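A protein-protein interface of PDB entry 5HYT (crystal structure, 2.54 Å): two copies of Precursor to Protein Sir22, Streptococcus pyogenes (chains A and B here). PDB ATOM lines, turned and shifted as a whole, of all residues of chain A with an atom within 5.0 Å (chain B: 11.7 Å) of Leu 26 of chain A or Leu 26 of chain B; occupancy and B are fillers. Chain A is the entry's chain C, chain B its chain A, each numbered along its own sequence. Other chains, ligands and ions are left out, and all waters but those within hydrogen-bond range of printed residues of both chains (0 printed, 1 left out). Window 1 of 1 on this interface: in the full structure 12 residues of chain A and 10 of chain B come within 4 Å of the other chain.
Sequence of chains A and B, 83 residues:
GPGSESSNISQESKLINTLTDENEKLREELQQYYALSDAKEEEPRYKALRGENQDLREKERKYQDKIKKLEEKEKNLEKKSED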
ATOM      1  N   GLU A  22      20.688   9.085 -26.818  1.00  0.00           N
ATOM      2  CA  GLU A  22      20.389   8.671 -25.452  1.00  0.00           C
ATOM      3  C   GLU A  22      18.906   8.771 -25.213  1.00  0.00           C
ATOM      4  O   GLU A  22      18.301   7.863 -24.655  1.00  0.00           O
ATOM      5  CB  GLU A  22      21.116   9.542 -24.419  1.00  0.00           C
ATOM      6  CG  GLU A  22      21.062   8.994 -23.019  1.00  0.00           C
ATOM      7  CD  GLU A  22      21.746   9.887 -22.005  1.00  0.00           C
ATOM      8  OE1 GLU A  22      21.297  11.046 -21.840  1.00  0.00           O
ATOM      9  OE2 GLU A  22      22.715   9.420 -21.356  1.00  0.00           O
ATOM     10  N   ASN A  23      18.323   9.871 -25.678  1.00  0.00           N
ATOM     11  CA  ASN A  23      16.916  10.117 -25.472  1.00  0.00           C
ATOM     12  C   ASN A  23      16.100   8.994 -26.099  1.00  0.00           C
ATOM     13  O   ASN A  23      15.153   8.504 -25.492  1.00  0.00           O
ATOM     14  CB  ASN A  23      16.516  11.461 -26.062  1.00  0.00           C
ATOM     15  CG  ASN A  23      15.059  11.816 -25.780  1.00  0.00           C
ATOM     16  OD1 ASN A  23      14.135  11.357 -26.476  1.00  0.00           O
ATOM     17  ND2 ASN A  23      14.850  12.675 -24.784  1.00  0.00           N
ATOM     18  N   GLU A  24      16.515   8.541 -27.278  1.00  0.00           N
ATOM     19  CA  GLU A  24      15.804   7.467 -27.957  1.00  0.00           C
ATOM     20  C   GLU A  24      15.939   6.207 -27.151  1.00  0.00           C
ATOM     21  O   GLU A  24      14.945   5.504 -26.932  1.00  0.00           O
ATOM     22  CB  GLU A  24      16.320   7.231 -29.380  1.00  0.00           C
ATOM     23  CG  GLU A  24      15.433   6.269 -30.170  1.00  0.00           C
ATOM     24  CD  GLU A  24      16.002   5.909 -31.532  1.00  0.00           C
ATOM     25  OE1 GLU A  24      17.154   6.310 -31.803  1.00  0.00           O
ATOM     26  OE2 GLU A  24      15.291   5.243 -32.331  1.00  0.00           O
ATOM     27  N   LYS A  25      17.163   5.901 -26.720  1.00  0.00           N
ATOM     28  CA  LYS A  25      17.379   4.652 -26.005  1.00  0.00           C
ATOM     29  C   LYS A  25      16.734   4.618 -24.614  1.00  0.00           C
ATOM     30  O   LYS A  25      16.276   3.579 -24.186  1.00  0.00           O
ATOM     31  CB  LYS A  25      18.870   4.326 -25.917  1.00  0.00           C
ATOM     32  CG  LYS A  25      19.327   3.608 -27.179  1.00  0.00           C
ATOM     33  CD  LYS A  25      20.795   3.703 -27.490  1.00  0.00           C
ATOM     34  CE  LYS A  25      21.143   2.674 -28.555  1.00  0.00           C
ATOM     35  NZ  LYS A  25      22.612   2.504 -28.720  1.00  0.00           N
ATOM     36  N   LEU A  26      16.632   5.763 -23.961  1.00  0.00           N
ATOM     37  CA  LEU A  26      16.059   5.834 -22.642  1.00  0.00           C
ATOM     38  C   LEU A  26      14.565   5.555 -22.834  1.00  0.00           C
ATOM     39  O   LEU A  26      13.924   4.874 -22.032  1.00  0.00           O
ATOM     40  CB  LEU A  26      16.344   7.201 -22.024  1.00  0.00           C
ATOM     41  CG  LEU A  26      17.098   7.305 -20.701  1.00  0.00           C
ATOM     42  CD1 LEU A  26      18.325   6.400 -20.612  1.00  0.00           C
ATOM     43  CD2 LEU A  26      17.529   8.749 -20.566  1.00  0.00           C
ATOM     44  N   ARG A  27      14.008   6.079 -23.921  1.00  0.00           N
ATOM     45  CA  ARG A  27      12.609   5.807 -24.249  1.00  0.00           C
ATOM     46  C   ARG A  27      12.371   4.321 -24.587  1.00  0.00           C
ATOM     47  O   ARG A  27      11.359   3.741 -24.191  1.00  0.00           O
ATOM     48  CB  ARG A  27      12.172   6.686 -25.401  1.00  0.00           C
ATOM     49  CG  ARG A  27      11.994   8.128 -24.990  1.00  0.00           C
ATOM     50  CD  ARG A  27      11.710   9.047 -26.176  1.00  0.00           C
ATOM     51  NE  ARG A  27      11.465  10.390 -25.670  1.00  0.00           N
ATOM     52  CZ  ARG A  27      10.314  10.760 -25.123  1.00  0.00           C
ATOM     53  NH1 ARG A  27       9.313   9.891 -25.027  1.00  0.00           N
ATOM     54  NH2 ARG A  27      10.163  11.990 -24.660  1.00  0.00           N
ATOM     55  N   GLU A  28      13.304   3.694 -25.293  1.00  0.00           N
ATOM     56  CA  GLU A  28      13.170   2.267 -25.534  1.00  0.00           C
ATOM     57  C   GLU A  28      13.259   1.495 -24.224  1.00  0.00           C
ATOM     58  O   GLU A  28      12.507   0.544 -23.999  1.00  0.00           O
ATOM     59  CB  GLU A  28      14.233   1.775 -26.503  1.00  0.00           C
ATOM     60  CG  GLU A  28      14.062   2.335 -27.884  1.00  0.00           C
ATOM     61  CD  GLU A  28      15.110   1.842 -28.851  1.00  0.00           C
ATOM     62  OE1 GLU A  28      16.093   1.209 -28.407  1.00  0.00           O
ATOM     63  OE2 GLU A  28      14.939   2.075 -30.066  1.00  0.00           O
ATOM     64  N   GLU A  29      14.169   1.935 -23.360  1.00  0.00           N
ATOM     65  CA  GLU A  29      14.413   1.267 -22.099  1.00  0.00           C
ATOM     66  C   GLU A  29      13.153   1.301 -21.245  1.00  0.00           C
ATOM     67  O   GLU A  29      12.827   0.312 -20.577  1.00  0.00           O
ATOM     68  CB  GLU A  29      15.586   1.914 -21.341  1.00  0.00           C
ATOM     69  CG  GLU A  29      16.382   0.926 -20.465  1.00  0.00           C
ATOM     70  CD  GLU A  29      17.423   1.593 -19.557  1.00  0.00           C
ATOM     71  OE1 GLU A  29      18.112   2.525 -20.040  1.00  0.00           O
ATOM     72  OE2 GLU A  29      17.561   1.166 -18.373  1.00  0.00           O
ATOM     73  N   LEU A  30      12.461   2.441 -21.256  1.00  0.00           N
ATOM     74  CA  LEU A  30      11.239   2.552 -20.480  1.00  0.00           C
ATOM     75  C   LEU A  30      10.181   1.576 -20.973  1.00  0.00           C
ATOM     76  O   LEU A  30       9.466   0.988 -20.175  1.00  0.00           O
ATOM     77  CB  LEU A  30      10.694   3.983 -20.506  1.00  0.00           C
ATOM     78  CG  LEU A  30      11.334   4.876 -19.444  1.00  0.00           C
ATOM     79  CD1 LEU A  30      10.989   6.336 -19.654  1.00  0.00           C
ATOM     80  CD2 LEU A  30      10.947   4.405 -18.025  1.00  0.00           C
ATOM     81  N   ASN B  17      20.222  21.906 -23.904  1.00  0.00           N
ATOM     82  CA  ASN B  17      19.494  21.957 -22.649  1.00  0.00           C
ATOM     83  C   ASN B  17      18.162  21.217 -22.692  1.00  0.00           C
ATOM     84  O   ASN B  17      17.805  20.547 -21.729  1.00  0.00           O
ATOM     85  CB  ASN B  17      19.276  23.404 -22.220  1.00  0.00           C
ATOM     86  CG  ASN B  17      20.527  24.036 -21.631  1.00  0.00           C
ATOM     87  OD1 ASN B  17      21.505  23.342 -21.314  1.00  0.00           O
ATOM     88  ND2 ASN B  17      20.493  25.354 -21.454  1.00  0.00           N
ATOM     89  N   THR B  18      17.438  21.333 -23.803  1.00  0.00           N
ATOM     90  CA  THR B  18      16.179  20.620 -23.974  1.00  0.00           C
ATOM     91  C   THR B  18      16.403  19.116 -23.843  1.00  0.00           C
ATOM     92  O   THR B  18      15.723  18.446 -23.075  1.00  0.00           O
ATOM     93  CB  THR B  18      15.525  20.934 -25.355  1.00  0.00           C
ATOM     94  OG1 THR B  18      14.937  22.247 -25.339  1.00  0.00           O
ATOM     95  CG2 THR B  18      14.454  19.912 -25.706  1.00  0.00           C
ATOM     96  N   LEU B  19      17.383  18.591 -24.563  1.00  0.00           N
ATOM     97  CA  LEU B  19      17.647  17.160 -24.542  1.00  0.00           C
ATOM     98  C   LEU B  19      18.202  16.722 -23.196  1.00  0.00           C
ATOM     99  O   LEU B  19      17.887  15.633 -22.709  1.00  0.00           O
ATOM    100  CB  LEU B  19      18.599  16.778 -25.675  1.00  0.00           C
ATOM    101  CG  LEU B  19      17.918  16.867 -27.052  1.00  0.00           C
ATOM    102  CD1 LEU B  19      18.858  16.576 -28.220  1.00  0.00           C
ATOM    103  CD2 LEU B  19      16.724  15.914 -27.074  1.00  0.00           C
ATOM    104  N   THR B  20      19.027  17.566 -22.590  1.00  0.00           N
ATOM    105  CA  THR B  20      19.601  17.223 -21.296  1.00  0.00           C
ATOM    106  C   THR B  20      18.515  17.117 -20.226  1.00  0.00           C
ATOM    107  O   THR B  20      18.502  16.178 -19.443  1.00  0.00           O
ATOM    108  CB  THR B  20      20.686  18.258 -20.875  1.00  0.00           C
ATOM    109  OG1 THR B  20      21.791  18.174 -21.786  1.00  0.00           O
ATOM    110  CG2 THR B  20      21.213  17.978 -19.483  1.00  0.00           C
ATOM    111  N   ASP B  21      17.589  18.065 -20.220  1.00  0.00           N
ATOM    112  CA  ASP B  21      16.513  18.077 -19.248  1.00  0.00           C
ATOM    113  C   ASP B  21      15.544  16.932 -19.492  1.00  0.00           C
ATOM    114  O   ASP B  21      15.073  16.293 -18.548  1.00  0.00           O
ATOM    115  CB  ASP B  21      15.783  19.414 -19.295  1.00  0.00           C
ATOM    116  CG  ASP B  21      16.667  20.576 -18.879  1.00  0.00           C
ATOM    117  OD1 ASP B  21      17.653  20.349 -18.143  1.00  0.00           O
ATOM    118  OD2 ASP B  21      16.388  21.716 -19.304  1.00  0.00           O
ATOM    119  N   GLU B  22      15.271  16.657 -20.763  1.00  0.00           N
ATOM    120  CA  GLU B  22      14.325  15.613 -21.106  1.00  0.00           C
ATOM    121  C   GLU B  22      14.917  14.261 -20.709  1.00  0.00           C
ATOM    122  O   GLU B  22      14.220  13.413 -20.174  1.00  0.00           O
ATOM    123  CB  GLU B  22      13.970  15.666 -22.596  1.00  0.00           C
ATOM    124  CG  GLU B  22      12.750  14.852 -22.965  1.00  0.00           C
ATOM    125  CD  GLU B  22      12.389  14.924 -24.443  1.00  0.00           C
ATOM    126  OE1 GLU B  22      12.592  13.918 -25.163  1.00  0.00           O
ATOM    127  OE2 GLU B  22      11.875  15.980 -24.885  1.00  0.00           O
ATOM    128  N   ASN B  23      16.194  14.058 -20.995  1.00  0.00           N
ATOM    129  CA  ASN B  23      16.879  12.830 -20.630  1.00  0.00           C
ATOM    130  C   ASN B  23      16.933  12.655 -19.127  1.00  0.00           C
ATOM    131  O   ASN B  23      16.882  11.544 -18.610  1.00  0.00           O
ATOM    132  CB  ASN B  23      18.288  12.799 -21.197  1.00  0.00           C
ATOM    133  CG  ASN B  23      18.290  12.544 -22.670  1.00  0.00           C
ATOM    134  OD1 ASN B  23      17.251  12.634 -23.306  1.00  0.00           O
ATOM    135  ND2 ASN B  23      19.456  12.200 -23.226  1.00  0.00           N
ATOM    136  N   GLU B  24      17.073  13.763 -18.426  1.00  0.00           N
ATOM    137  CA  GLU B  24      17.137  13.706 -16.984  1.00  0.00           C
ATOM    138  C   GLU B  24      15.794  13.194 -16.485  1.00  0.00           C
ATOM    139  O   GLU B  24      15.724  12.288 -15.659  1.00  0.00           O
ATOM    140  CB  GLU B  24      17.452  15.078 -16.397  1.00  0.00           C
ATOM    141  CG  GLU B  24      17.792  15.062 -14.918  1.00  0.00           C
ATOM    142  CD  GLU B  24      17.913  16.466 -14.357  1.00  0.00           C
ATOM    143  OE1 GLU B  24      17.609  17.423 -15.101  1.00  0.00           O
ATOM    144  OE2 GLU B  24      18.317  16.619 -13.187  1.00  0.00           O
ATOM    145  N   LYS B  25      14.723  13.744 -17.022  1.00  0.00           N
ATOM    146  CA  LYS B  25      13.385  13.417 -16.527  1.00  0.00           C
ATOM    147  C   LYS B  25      13.072  11.957 -16.803  1.00  0.00           C
ATOM    148  O   LYS B  25      12.462  11.258 -15.999  1.00  0.00           O
ATOM    149  CB  LYS B  25      12.379  14.309 -17.222  1.00  0.00           C
ATOM    150  CG  LYS B  25      12.327  15.728 -16.705  1.00  0.00           C
ATOM    151  CD  LYS B  25      12.123  16.638 -17.905  1.00  0.00           C
ATOM    152  CE  LYS B  25      10.696  16.966 -18.224  1.00  0.00           C
ATOM    153  NZ  LYS B  25      10.735  17.699 -19.523  1.00  0.00           N
ATOM    154  N   LEU B  26      13.610  11.482 -17.909  1.00  0.00           N
ATOM    155  CA  LEU B  26      13.411  10.129 -18.370  1.00  0.00           C
ATOM    156  C   LEU B  26      14.151   9.152 -17.480  1.00  0.00           C
ATOM    157  O   LEU B  26      13.640   8.088 -17.148  1.00  0.00           O
ATOM    158  CB  LEU B  26      13.888  10.045 -19.818  1.00  0.00           C
ATOM    159  CG  LEU B  26      12.936   9.588 -20.906  1.00  0.00           C
ATOM    160  CD1 LEU B  26      11.564  10.191 -20.715  1.00  0.00           C
ATOM    161  CD2 LEU B  26      13.538  10.089 -22.218  1.00  0.00           C
ATOM    162  N   ARG B  27      15.366   9.537 -17.099  1.00  0.00           N
ATOM    163  CA  ARG B  27      16.207   8.749 -16.200  1.00  0.00           C
ATOM    164  C   ARG B  27      15.592   8.649 -14.809  1.00  0.00           C
ATOM    165  O   ARG B  27      15.693   7.611 -14.157  1.00  0.00           O
ATOM    166  CB  ARG B  27      17.612   9.354 -16.115  1.00  0.00           C
ATOM    167  CG  ARG B  27      18.527   8.594 -15.211  1.00  0.00           C
ATOM    168  CD  ARG B  27      19.051   7.353 -15.900  1.00  0.00           C
ATOM    169  NE  ARG B  27      19.896   7.682 -17.045  1.00  0.00           N
ATOM    170  CZ  ARG B  27      20.390   6.771 -17.880  1.00  0.00           C
ATOM    171  NH1 ARG B  27      20.107   5.484 -17.694  1.00  0.00           N
ATOM    172  NH2 ARG B  27      21.160   7.138 -18.900  1.00  0.00           N
ATOM    173  N   GLU B  28      14.953   9.726 -14.361  1.00  0.00           N
ATOM    174  CA  GLU B  28      14.243   9.711 -13.087  1.00  0.00           C
ATOM    175  C   GLU B  28      13.124   8.697 -13.211  1.00  0.00           C
ATOM    176  O   GLU B  28      12.861   7.946 -12.299  1.00  0.00           O
ATOM    177  CB  GLU B  28      13.663  11.084 -12.769  1.00  0.00           C
ATOM    178  CG  GLU B  28      14.697  12.158 -12.581  1.00  0.00           C
ATOM    179  CD  GLU B  28      14.073  13.520 -12.388  1.00  0.00           C
ATOM    180  OE1 GLU B  28      12.842  13.639 -12.575  1.00  0.00           O
ATOM    181  OE2 GLU B  28      14.801  14.478 -12.042  1.00  0.00           O
ATOM    182  N   GLU B  29      12.473   8.675 -14.368  1.00  0.00           N
ATOM    183  CA  GLU B  29      11.362   7.773 -14.576  1.00  0.00           C
ATOM    184  C   GLU B  29      11.852   6.313 -14.539  1.00  0.00           C
ATOM    185  O   GLU B  29      11.240   5.440 -13.914  1.00  0.00           O
ATOM    186  CB  GLU B  29      10.662   8.090 -15.882  1.00  0.00           C
ATOM    187  CG  GLU B  29       9.196   8.014 -15.706  1.00  0.00           C
ATOM    188  CD  GLU B  29       8.666   9.280 -15.100  1.00  0.00           C
ATOM    189  OE1 GLU B  29       9.379  10.296 -15.227  1.00  0.00           O
ATOM    190  OE2 GLU B  29       7.580   9.272 -14.483  1.00  0.00           O
ATOM    191  N   LEU B  30      12.991   6.057 -15.168  1.00  0.00           N
ATOM    192  CA  LEU B  30      13.582   4.727 -15.115  1.00  0.00           C
ATOM    193  C   LEU B  30      13.912   4.356 -13.669  1.00  0.00           C
ATOM    194  O   LEU B  30      13.963   3.175 -13.312  1.00  0.00           O
ATOM    195  CB  LEU B  30      14.812   4.658 -15.983  1.00  0.00           C
ATOM    196  CG  LEU B  30      14.504   4.342 -17.437  1.00  0.00           C
ATOM    197  CD1 LEU B  30      15.696   4.655 -18.329  1.00  0.00           C
ATOM    198  CD2 LEU B  30      14.204   2.880 -17.524  1.00  0.00           C
ATOM    199  N   GLN B  31      14.141   5.368 -12.838  1.00  0.00           N
ATOM    200  CA  GLN B  31      14.564   5.132 -11.470  1.00  0.00           C
ATOM    201  C   GLN B  31      13.476   4.382 -10.711  1.00  0.00           C
ATOM    202  O   GLN B  31      13.759   3.478  -9.921  1.00  0.00           O
ATOM    203  CB  GLN B  31      14.841   6.453 -10.754  1.00  0.00           C
ATOM    204  CG  GLN B  31      16.207   7.044 -10.988  1.00  0.00           C
ATOM    205  CD  GLN B  31      17.305   6.092 -10.629  1.00  0.00           C
ATOM    206  OE1 GLN B  31      18.161   5.819 -11.463  1.00  0.00           O
ATOM    207  NE2 GLN B  31      17.283   5.554  -9.396  1.00  0.00           N
ATOM    208  N   GLN B  32      12.225   4.724 -10.990  1.00  0.00           N
ATOM    209  CA  GLN B  32      11.106   4.026 -10.369  1.00  0.00           C
ATOM    210  C   GLN B  32      11.122   2.532 -10.692  1.00  0.00           C
ATOM    211  O   GLN B  32      10.802   1.725  -9.833  1.00  0.00           O
ATOM    212  CB  GLN B  32       9.798   4.673 -10.771  1.00  0.00           C
ATOM    213  CG  GLN B  32       9.766   6.106 -10.296  1.00  0.00           C
ATOM    214  CD  GLN B  32       8.412   6.737 -10.367  1.00  0.00           C
ATOM    215  OE1 GLN B  32       7.614   6.420 -11.235  1.00  0.00           O
ATOM    216  NE2 GLN B  32       8.173   7.706  -9.493  1.00  0.00           N
ATOM    217  N   TYR B  33      11.502   2.164 -11.913  1.00  0.00           N
ATOM    218  CA  TYR B  33      11.612   0.756 -12.276  1.00  0.00           C
ATOM    219  C   TYR B  33      12.792   0.065 -11.612  1.00  0.00           C
ATOM    220  O   TYR B  33      12.695  -1.104 -11.231  1.00  0.00           O
ATOM    221  CB  TYR B  33      11.718   0.601 -13.795  1.00  0.00           C
ATOM    222  CG  TYR B  33      10.380   0.733 -14.491  1.00  0.00           C
ATOM    223  CD1 TYR B  33       9.422  -0.283 -14.402  1.00  0.00           C
ATOM    224  CD2 TYR B  33      10.075   1.861 -15.239  1.00  0.00           C
ATOM    225  CE1 TYR B  33       8.203  -0.166 -15.029  1.00  0.00           C
ATOM    226  CE2 TYR B  33       8.863   1.981 -15.877  1.00  0.00           C
ATOM    227  CZ  TYR B  33       7.928   0.966 -15.768  1.00  0.00           C
ATOM    228  OH  TYR B  33       6.715   1.085 -16.398  1.00  0.00           O
ATOM    229  N   TYR B  34      13.921   0.767 -11.518  1.00  0.00           N
ATOM    230  CA  TYR B  34      15.123   0.255 -10.853  1.00  0.00           C
ATOM    231  C   TYR B  34      14.849  -0.077  -9.377  1.00  0.00           C
ATOM    232  O   TYR B  34      15.335  -1.077  -8.838  1.00  0.00           O
ATOM    233  CB  TYR B  34      16.251   1.283 -10.941  1.00  0.00           C
ATOM    234  CG  TYR B  34      16.729   1.611 -12.349  1.00  0.00           C
ATOM    235  CD1 TYR B  34      16.628   0.685 -13.384  1.00  0.00           C
ATOM    236  CD2 TYR B  34      17.228   2.869 -12.646  1.00  0.00           C
ATOM    237  CE1 TYR B  34      17.060   0.987 -14.651  1.00  0.00           C
ATOM    238  CE2 TYR B  34      17.655   3.188 -13.920  1.00  0.00           C
ATOM    239  CZ  TYR B  34      17.567   2.250 -14.922  1.00  0.00           C
ATOM    240  OH  TYR B  34      17.998   2.581 -16.193  1.00  0.00           O
ATOM    241  N   ALA B  35      14.052   0.791  -8.761  1.00  0.00           N
ATOM    242  CA  ALA B  35      13.718   0.780  -7.349  1.00  0.00           C
ATOM    243  C   ALA B  35      12.998  -0.489  -6.929  1.00  0.00           C
ATOM    244  O   ALA B  35      13.094  -0.916  -5.772  1.00  0.00           O
ATOM    245  CB  ALA B  35      12.882   1.998  -7.017  1.00  0.00           C
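Glu 22 of chain A touches Arg 27 of chain B, and with the chains exchanged Arg 27 of chain A touches Glu 22 of chain B.
Leu 26 of chain B touches its own counterpart, Leu 26 of chain A.
Leu 26 of chain A touches Arg 27 of chain B, and with the chains exchanged Arg 27 of chain A touches Leu 26 of chain B.
Leu 30 of chain A touches its own counterpart, Leu 30 of chain B.
Positions printed for both chains: 22, 23, 24, 25, 26, 27, 28, 29 and 30.
Of the 16 pairs that touch across the chains among the printed residues, 13 have their exchanged pair printed and touching as well.
Printed residues of chain A that touch a printed residue of chain B: Glu 22, Asn 23, Leu 26, Arg 27, Glu 29 and Leu 30.
Hydrophobic or aromatic side chains of chain A that line the printed part of chain B: Leu 26 and Leu 30.
The side-chain carboxylate (OE1) of Glu 22 of chain B sits at hydrogen-bond distance from the side-chain amide nitrogen (ND2) of Asn 23 of chain A, 2.6 Å away.
The side-chain carboxylate (OE1) of Glu 22 of chain B lies within salt-bridge range of the guanidinium group (NH2) of Arg 27 of chain A (3.1 Å).
ND2 of Asn 23 of chain B is in hydrogen-bond range of OE1 of Glu 22 of chain A, 2.6 Å away.
The side-chain amide oxygen (OD1) of Asn 23 of chain B lies within hydrogen-bond range of the side-chain amide nitrogen (ND2) of Asn 23 of chain A.
NH2 of Arg 27 of chain B lies within salt-bridge range of OE2 of Glu 22 of chain A (3.7 Å).
The side-chain hydroxyl (OH) of Tyr 34 of chain B sits at hydrogen-bond distance from the side-chain carboxylate (OE2) of Glu 29 of chain A, 2.6 Å away.
Among the printed residues, pairs that only touch across the chains: Asn 23 of chain A with Leu 26 of chain B, Leu 26 of chain A with Asn 23 of chain B, Leu 26 of chain A with Leu 26 of chain B, Leu 26 of chain A with Arg 27 of chain B, Leu 26 of chain A with Leu 30 of chain B, Arg 27 of chain A with Leu 26 of chain B, Glu 29 of chain A with Leu 30 of chain B, Leu 30 of chain A with Leu 26 of chain B, Leu 30 of chain A with Leu 30 of chain B and Leu 30 of chain A with Tyr 33 of chain B.
The backbone carbonyl oxygen (O) of Leu 19 of chain B sits close to the side-chain amide oxygen (OD1) of Asn 23 of chain B (3.1 Å).
NE of Arg 27 of chain A sits at hydrogen-bond distance from OD1 of Asn 23 of chain A (3.0 Å).
Leu 26 of chain A touches just these residues of chain B: Asn 23, Leu 26, Arg 27 and Leu 30.
Of the printed residues of chain A, Leu 26 of chain B touches Asn 23 (3.9 Å), Leu 26 (3.9 Å), Arg 27 (3.7 Å) and Leu 30 (3.99 Å).
Glu 22 of chain A touches just these residues of chain B: Asn 23 and Arg 27.
Asn 23 of chain A touches just these residues of chain B: Glu 22, Asn 23 and Leu 26.
Arg 27 of chain A touches just these residues of chain B: Glu 22 and Leu 26.
No residue of chain B comes within 4 Å of Glu 28 of chain A.
Glu 29 of chain A touches just these residues of chain B: Leu 30 (3.6 Å) and Tyr 34 (2.6 Å).
Of the printed residues of chain B, Leu 30 of chain A touches Leu 26, Leu 30 and Tyr 33.
Printed residues of chain A within 4 Å of Asn 23 of chain B: Glu 22 (2.6 Å), Asn 23 (2.8 Å) and Leu 26 (3.5 Å).
Glu 29 of chain B touches none of the printed residues of chain A.
The nearest residue of chain B that does not touch Leu 26 of chain A is Glu 24 of chain B (5.5 Å).
The nearest printed residue of chain A that does not touch Leu 26 of chain B is Glu 22 of chain A (5.8 Å).
The nearest printed residue of chain A that does not touch Arg 27 of chain B is Glu 29 of chain A (4.3 Å).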
